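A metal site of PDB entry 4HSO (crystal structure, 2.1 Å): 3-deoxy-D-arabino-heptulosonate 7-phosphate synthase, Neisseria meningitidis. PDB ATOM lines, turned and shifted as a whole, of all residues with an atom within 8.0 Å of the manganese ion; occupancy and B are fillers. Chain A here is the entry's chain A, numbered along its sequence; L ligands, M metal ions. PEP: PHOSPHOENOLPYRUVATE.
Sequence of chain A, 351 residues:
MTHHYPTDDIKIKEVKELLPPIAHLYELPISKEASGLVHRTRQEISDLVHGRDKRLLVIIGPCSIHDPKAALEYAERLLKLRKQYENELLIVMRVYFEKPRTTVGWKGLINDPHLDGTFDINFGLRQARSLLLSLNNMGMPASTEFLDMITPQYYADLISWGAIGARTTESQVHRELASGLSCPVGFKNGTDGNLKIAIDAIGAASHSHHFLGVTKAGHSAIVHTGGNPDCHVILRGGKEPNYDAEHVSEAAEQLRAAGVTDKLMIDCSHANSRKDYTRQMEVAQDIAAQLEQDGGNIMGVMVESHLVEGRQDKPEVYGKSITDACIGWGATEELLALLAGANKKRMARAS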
ATOM      1  N   GLY A  61      -1.966  18.113  21.412  1.00  0.00           N
ATOM      2  CA  GLY A  61      -1.755  18.129  19.969  1.00  0.00           C
ATOM      3  C   GLY A  61      -0.967  16.923  19.491  1.00  0.00           C
ATOM      4  O   GLY A  61      -0.813  15.962  20.214  1.00  0.00           O
ATOM      5  N   PRO A  62      -0.483  16.959  18.252  1.00  0.00           N
ATOM      6  CA  PRO A  62       0.205  15.820  17.654  1.00  0.00           C
ATOM      7  C   PRO A  62       1.466  15.397  18.385  1.00  0.00           C
ATOM      8  O   PRO A  62       2.097  16.197  19.044  1.00  0.00           O
ATOM      9  CB  PRO A  62       0.538  16.326  16.264  1.00  0.00           C
ATOM     10  CG  PRO A  62      -0.582  17.246  15.933  1.00  0.00           C
ATOM     11  CD  PRO A  62      -0.905  17.939  17.237  1.00  0.00           C
ATOM     12  N   CYS A  63       1.779  14.117  18.303  1.00  0.00           N
ATOM     13  CA  CYS A  63       3.021  13.636  18.781  1.00  0.00           C
ATOM     14  C   CYS A  63       4.113  14.491  18.076  1.00  0.00           C
ATOM     15  O   CYS A  63       4.950  15.101  18.704  1.00  0.00           O
ATOM     16  CB  CYS A  63       3.165  12.136  18.465  1.00  0.00           C
ATOM     17  SG  CYS A  63       4.792  11.441  18.984  1.00  0.00           S
ATOM     18  N   SER A  64       4.027  14.542  16.762  1.00  0.00           N
ATOM     19  CA  SER A  64       4.976  15.290  15.955  1.00  0.00           C
ATOM     20  C   SER A  64       4.286  16.027  14.867  1.00  0.00           C
ATOM     21  O   SER A  64       3.218  15.578  14.371  1.00  0.00           O
ATOM     22  CB  SER A  64       5.994  14.343  15.356  1.00  0.00           C
ATOM     23  OG  SER A  64       5.402  13.393  14.508  1.00  0.00           O
ATOM     24  N   ARG A  94       0.520  21.367  21.198  1.00  0.00           N
ATOM     25  CA  ARG A  94       1.779  20.648  21.042  1.00  0.00           C
ATOM     26  C   ARG A  94       2.257  20.894  19.594  1.00  0.00           C
ATOM     27  O   ARG A  94       1.559  20.468  18.659  1.00  0.00           O
ATOM     28  CB  ARG A  94       1.624  19.130  21.154  1.00  0.00           C
ATOM     29  CG  ARG A  94       1.500  18.591  22.549  1.00  0.00           C
ATOM     30  CD  ARG A  94       1.455  17.063  22.601  1.00  0.00           C
ATOM     31  NE  ARG A  94       2.523  16.373  21.875  1.00  0.00           N
ATOM     32  CZ  ARG A  94       3.500  15.678  22.433  1.00  0.00           C
ATOM     33  NH1 ARG A  94       3.629  15.633  23.741  1.00  0.00           N
ATOM     34  NH2 ARG A  94       4.409  15.095  21.672  1.00  0.00           N
ATOM     35  N   TYR A  96       5.653  19.959  18.270  1.00  0.00           N
ATOM     36  CA  TYR A  96       6.902  19.237  18.424  1.00  0.00           C
ATOM     37  C   TYR A  96       7.559  18.962  17.066  1.00  0.00           C
ATOM     38  O   TYR A  96       7.016  18.206  16.254  1.00  0.00           O
ATOM     39  CB  TYR A  96       6.694  17.936  19.142  1.00  0.00           C
ATOM     40  CG  TYR A  96       6.542  18.050  20.620  1.00  0.00           C
ATOM     41  CD1 TYR A  96       5.707  19.015  21.190  1.00  0.00           C
ATOM     42  CD2 TYR A  96       7.168  17.165  21.472  1.00  0.00           C
ATOM     43  CE1 TYR A  96       5.547  19.111  22.562  1.00  0.00           C
ATOM     44  CE2 TYR A  96       6.960  17.230  22.868  1.00  0.00           C
ATOM     45  CZ  TYR A  96       6.168  18.233  23.387  1.00  0.00           C
ATOM     46  OH  TYR A  96       5.967  18.334  24.805  1.00  0.00           O
ATOM     47  N   LYS A  99      12.097  15.023  17.651  1.00  0.00           N
ATOM     48  CA  LYS A  99      11.655  13.751  18.198  1.00  0.00           C
ATOM     49  C   LYS A  99      12.827  12.801  18.550  1.00  0.00           C
ATOM     50  O   LYS A  99      13.646  12.450  17.661  1.00  0.00           O
ATOM     51  CB  LYS A  99      10.722  13.038  17.232  1.00  0.00           C
ATOM     52  CG  LYS A  99       9.536  13.860  16.816  1.00  0.00           C
ATOM     53  CD  LYS A  99       8.705  14.346  17.997  1.00  0.00           C
ATOM     54  CE  LYS A  99       8.060  13.176  18.797  1.00  0.00           C
ATOM     55  NZ  LYS A  99       7.290  13.715  19.941  1.00  0.00           N
ATOM     56  N   PRO A 100      12.863  12.307  19.794  1.00  0.00           N
ATOM     57  CA  PRO A 100      13.970  11.448  20.186  1.00  0.00           C
ATOM     58  C   PRO A 100      13.614   9.990  19.921  1.00  0.00           C
ATOM     59  O   PRO A 100      12.605   9.510  20.417  1.00  0.00           O
ATOM     60  CB  PRO A 100      14.116  11.741  21.687  1.00  0.00           C
ATOM     61  CG  PRO A 100      12.762  12.157  22.152  1.00  0.00           C
ATOM     62  CD  PRO A 100      12.059  12.757  20.939  1.00  0.00           C
ATOM     63  N   GLU A 145       9.252  20.393  22.358  1.00  0.00           N
ATOM     64  CA  GLU A 145      10.352  19.799  23.101  1.00  0.00           C
ATOM     65  C   GLU A 145      11.622  20.357  22.590  1.00  0.00           C
ATOM     66  O   GLU A 145      11.899  20.352  21.409  1.00  0.00           O
ATOM     67  CB  GLU A 145      10.397  18.280  23.021  1.00  0.00           C
ATOM     68  CG  GLU A 145      11.481  17.682  23.936  1.00  0.00           C
ATOM     69  CD  GLU A 145      11.801  16.218  23.699  1.00  0.00           C
ATOM     70  OE1 GLU A 145      10.902  15.460  23.314  1.00  0.00           O
ATOM     71  OE2 GLU A 145      12.939  15.778  24.036  1.00  0.00           O
ATOM     72  N   ARG A 167      14.313  11.334  28.113  1.00  0.00           N
ATOM     73  CA  ARG A 167      15.595  10.865  27.738  1.00  0.00           C
ATOM     74  C   ARG A 167      16.720  11.842  27.992  1.00  0.00           C
ATOM     75  O   ARG A 167      17.825  11.509  27.844  1.00  0.00           O
ATOM     76  CB  ARG A 167      15.592  10.315  26.313  1.00  0.00           C
ATOM     77  CG  ARG A 167      14.713   9.077  26.144  1.00  0.00           C
ATOM     78  CD  ARG A 167      14.342   8.762  24.717  1.00  0.00           C
ATOM     79  NE  ARG A 167      13.314   7.726  24.644  1.00  0.00           N
ATOM     80  CZ  ARG A 167      12.003   7.907  24.789  1.00  0.00           C
ATOM     81  NH1 ARG A 167      11.488   9.087  25.010  1.00  0.00           N
ATOM     82  NH2 ARG A 167      11.198   6.891  24.702  1.00  0.00           N
ATOM     83  N   LYS A 188      10.394  15.780  32.340  1.00  0.00           N
ATOM     84  CA  LYS A 188       9.713  14.481  32.460  1.00  0.00           C
ATOM     85  C   LYS A 188      10.515  13.595  33.323  1.00  0.00           C
ATOM     86  O   LYS A 188      11.743  13.711  33.322  1.00  0.00           O
ATOM     87  CB  LYS A 188       9.561  13.834  31.077  1.00  0.00           C
ATOM     88  CG  LYS A 188       8.610  14.631  30.221  1.00  0.00           C
ATOM     89  CD  LYS A 188       8.157  13.926  28.976  1.00  0.00           C
ATOM     90  CE  LYS A 188       6.643  14.153  28.814  1.00  0.00           C
ATOM     91  NZ  LYS A 188       6.129  13.345  27.697  1.00  0.00           N
ATOM     92  N   ASP A 267       1.060  13.428  32.091  1.00  0.00           N
ATOM     93  CA  ASP A 267       0.985  13.115  30.697  1.00  0.00           C
ATOM     94  C   ASP A 267      -0.008  11.940  30.631  1.00  0.00           C
ATOM     95  O   ASP A 267       0.200  10.951  31.263  1.00  0.00           O
ATOM     96  CB  ASP A 267       2.361  12.701  30.162  1.00  0.00           C
ATOM     97  CG  ASP A 267       2.380  12.413  28.654  1.00  0.00           C
ATOM     98  OD1 ASP A 267       1.353  12.426  27.991  1.00  0.00           O
ATOM     99  OD2 ASP A 267       3.497  12.130  28.116  1.00  0.00           O
ATOM    100  N   SER A 269      -0.406  10.208  27.899  1.00  0.00           N
ATOM    101  CA  SER A 269       0.043   9.354  26.806  1.00  0.00           C
ATOM    102  C   SER A 269       1.346   8.604  27.166  1.00  0.00           C
ATOM    103  O   SER A 269       1.607   8.395  28.359  1.00  0.00           O
ATOM    104  CB  SER A 269       0.233  10.187  25.496  1.00  0.00           C
ATOM    105  OG  SER A 269       0.270   9.344  24.365  1.00  0.00           O
ATOM    106  N   HIS A 270       2.132   8.219  26.164  1.00  0.00           N
ATOM    107  CA  HIS A 270       3.367   7.468  26.366  1.00  0.00           C
ATOM    108  C   HIS A 270       3.219   6.346  27.468  1.00  0.00           C
ATOM    109  O   HIS A 270       2.359   5.498  27.342  1.00  0.00           O
ATOM    110  CB  HIS A 270       4.475   8.464  26.635  1.00  0.00           C
ATOM    111  CG  HIS A 270       4.527   9.515  25.579  1.00  0.00           C
ATOM    112  ND1 HIS A 270       3.936  10.749  25.731  1.00  0.00           N
ATOM    113  CD2 HIS A 270       4.984   9.481  24.299  1.00  0.00           C
ATOM    114  CE1 HIS A 270       4.088  11.458  24.635  1.00  0.00           C
ATOM    115  NE2 HIS A 270       4.715  10.704  23.754  1.00  0.00           N
ATOM    116  N   MET A 302      -1.051  16.574  29.663  1.00  0.00           N
ATOM    117  CA  MET A 302      -0.534  16.480  28.344  1.00  0.00           C
ATOM    118  C   MET A 302      -1.273  15.402  27.596  1.00  0.00           C
ATOM    119  O   MET A 302      -1.552  14.355  28.165  1.00  0.00           O
ATOM    120  CB  MET A 302       0.988  16.176  28.427  1.00  0.00           C
ATOM    121  CG  MET A 302       1.631  16.004  27.073  1.00  0.00           C
ATOM    122  SD  MET A 302       3.459  15.905  27.103  1.00  0.00           S
ATOM    123  CE  MET A 302       3.814  16.883  28.562  1.00  0.00           C
ATOM    124  N   GLU A 304      -1.909  13.501  23.548  1.00  0.00           N
ATOM    125  CA  GLU A 304      -1.485  13.311  22.150  1.00  0.00           C
ATOM    126  C   GLU A 304      -2.736  13.120  21.305  1.00  0.00           C
ATOM    127  O   GLU A 304      -3.458  12.118  21.449  1.00  0.00           O
ATOM    128  CB  GLU A 304      -0.472  12.161  22.021  1.00  0.00           C
ATOM    129  CG  GLU A 304       0.903  12.537  22.561  1.00  0.00           C
ATOM    130  CD  GLU A 304       1.986  11.557  22.222  1.00  0.00           C
ATOM    131  OE1 GLU A 304       1.751  10.336  22.381  1.00  0.00           O
ATOM    132  OE2 GLU A 304       3.076  12.025  21.745  1.00  0.00           O
ATOM    133  N   SER A 321      -1.094  10.834  12.549  1.00  0.00           N
ATOM    134  CA  SER A 321       0.281  10.787  13.044  1.00  0.00           C
ATOM    135  C   SER A 321       1.196   9.790  12.341  1.00  0.00           C
ATOM    136  O   SER A 321       0.747   8.750  11.947  1.00  0.00           O
ATOM    137  CB  SER A 321       0.276  10.476  14.566  1.00  0.00           C
ATOM    138  OG  SER A 321       1.614  10.391  15.066  1.00  0.00           O
ATOM    139  N   THR A 323       4.187   9.337  14.036  1.00  0.00           N
ATOM    140  CA  THR A 323       4.957   8.881  15.218  1.00  0.00           C
ATOM    141  C   THR A 323       4.046   8.116  16.183  1.00  0.00           C
ATOM    142  O   THR A 323       3.482   7.131  15.779  1.00  0.00           O
ATOM    143  CB  THR A 323       5.806  10.023  15.805  1.00  0.00           C
ATOM    144  OG1 THR A 323       5.031  11.206  15.994  1.00  0.00           O
ATOM    145  CG2 THR A 323       6.972  10.330  14.783  1.00  0.00           C
ATOM    146  N   ASP A 324       3.942   8.506  17.450  1.00  0.00           N
ATOM    147  CA  ASP A 324       3.016   7.817  18.355  1.00  0.00           C
ATOM    148  C   ASP A 324       1.583   8.022  17.915  1.00  0.00           C
ATOM    149  O   ASP A 324       1.246   9.050  17.308  1.00  0.00           O
ATOM    150  CB  ASP A 324       3.180   8.258  19.828  1.00  0.00           C
ATOM    151  CG  ASP A 324       4.592   8.115  20.323  1.00  0.00           C
ATOM    152  OD1 ASP A 324       5.246   7.174  19.924  1.00  0.00           O
ATOM    153  OD2 ASP A 324       5.048   9.048  21.074  1.00  0.00           O
ATOM    154  N   ALA A 325       0.719   7.072  18.275  1.00  0.00           N
ATOM    155  CA  ALA A 325      -0.658   7.071  17.858  1.00  0.00           C
ATOM    156  C   ALA A 325      -1.441   8.126  18.661  1.00  0.00           C
ATOM    157  O   ALA A 325      -1.208   8.301  19.801  1.00  0.00           O
ATOM    158  CB  ALA A 325      -1.265   5.699  18.043  1.00  0.00           C
ATOM    159  N   CYS A 326      -2.330   8.860  18.022  1.00  0.00           N
ATOM    160  CA  CYS A 326      -3.003   9.935  18.720  1.00  0.00           C
ATOM    161  C   CYS A 326      -4.470   9.593  18.794  1.00  0.00           C
ATOM    162  O   CYS A 326      -4.997   8.808  17.965  1.00  0.00           O
ATOM    163  CB  CYS A 326      -2.751  11.263  18.000  1.00  0.00           C
ATOM    164  SG  CYS A 326      -0.993  11.848  18.039  1.00  0.00           S
HETATM  165  C1  PEP L   1       6.553  13.388  23.697  1.00  0.00           C
HETATM  166  O1  PEP L   1       5.936  14.164  24.515  1.00  0.00           O
HETATM  167  O2' PEP L   1       6.179  13.187  22.503  1.00  0.00           O
HETATM  168  C2  PEP L   1       7.745  12.640  24.151  1.00  0.00           C
HETATM  169  C3  PEP L   1       8.819  12.433  23.374  1.00  0.00           C
HETATM  170  O2  PEP L   1       7.668  12.178  25.541  1.00  0.00           O
HETATM  171  P   PEP L   1       8.649  11.194  26.393  1.00  0.00           P
HETATM  172  O1P PEP L   1       8.819   9.963  25.618  1.00  0.00           O
HETATM  173  O2P PEP L   1       9.894  12.067  26.593  1.00  0.00           O
HETATM  174  O3P PEP L   1       7.681  10.892  27.578  1.00  0.00           O
HETATM  175 MN    MN M   1       4.869  10.924  21.527  1.00  0.00          MN
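The manganese ion is bound by the side-chain carboxylate of Asp 324 (1.9 Å), the side-chain carboxylate of Glu 304 (2.1 Å), a ring nitrogen (NE2) of His 270 (2.2 Å) and the side-chain sulfur of Cys 63 (2.6 Å).
The manganese ion has four donor atoms within binding distance.
Slightly farther from the manganese ion lies O2' of the ligand (2.8 Å).
The side-chain amino group of Lys 99 lies within salt-bridge range of an oxygen (O2') of the ligand (2.8 Å).
A ring nitrogen (NE2) of His 270 sits close to an oxygen (O2') of the ligand.
NZ of Lys 188 lies within salt-bridge range of O3P of the ligand (2.9 Å).
An oxygen (O2') of the ligand is in salt-bridge range of the guanidinium group of Arg 94 (2.7 Å).
The guanidinium group of Arg 167 lies within salt-bridge range of an oxygen (O1P) of the ligand (2.9 Å).
Four residues have an atom within 4 Å of the manganese ion: Cys 63, His 270, Glu 304 and Asp 324.
The nearest printed residue that does not touch the manganese ion is Lys 99 (4.02 Å).
The backbone carbonyl oxygen (O) of Asp 324 sits at hydrogen-bond distance from the side-chain sulfur (SG) of Cys 326 (3.7 Å).
The side-chain carboxylate (OE2) of Glu 304 sits close to the guanidinium group (NH2) of Arg 94, 3.3 Å away.
OE1 of Glu 304 sits at hydrogen-bond distance from OG of Ser 269, 2.7 Å away.
A ring nitrogen (ND1) of His 270 is in hydrogen-bond range of the side-chain carboxylate (OD2) of Asp 267 (2.8 Å).
The backbone carbonyl oxygen (O) of Asp 324 sits at hydrogen-bond distance from the side-chain hydroxyl (OG) of Ser 321 (2.6 Å).
The guanidinium group (NH2) of Arg 94 sits at hydrogen-bond distance from the backbone carbonyl oxygen (O) of Cys 63 (3.0 Å).
O of Cys 63 lies within hydrogen-bond range of NZ of Lys 99, 3.0 Å away.
The side-chain sulfur of Cys 63 sits close to the side-chain hydroxyl of Thr 323, 3.0 Å away.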
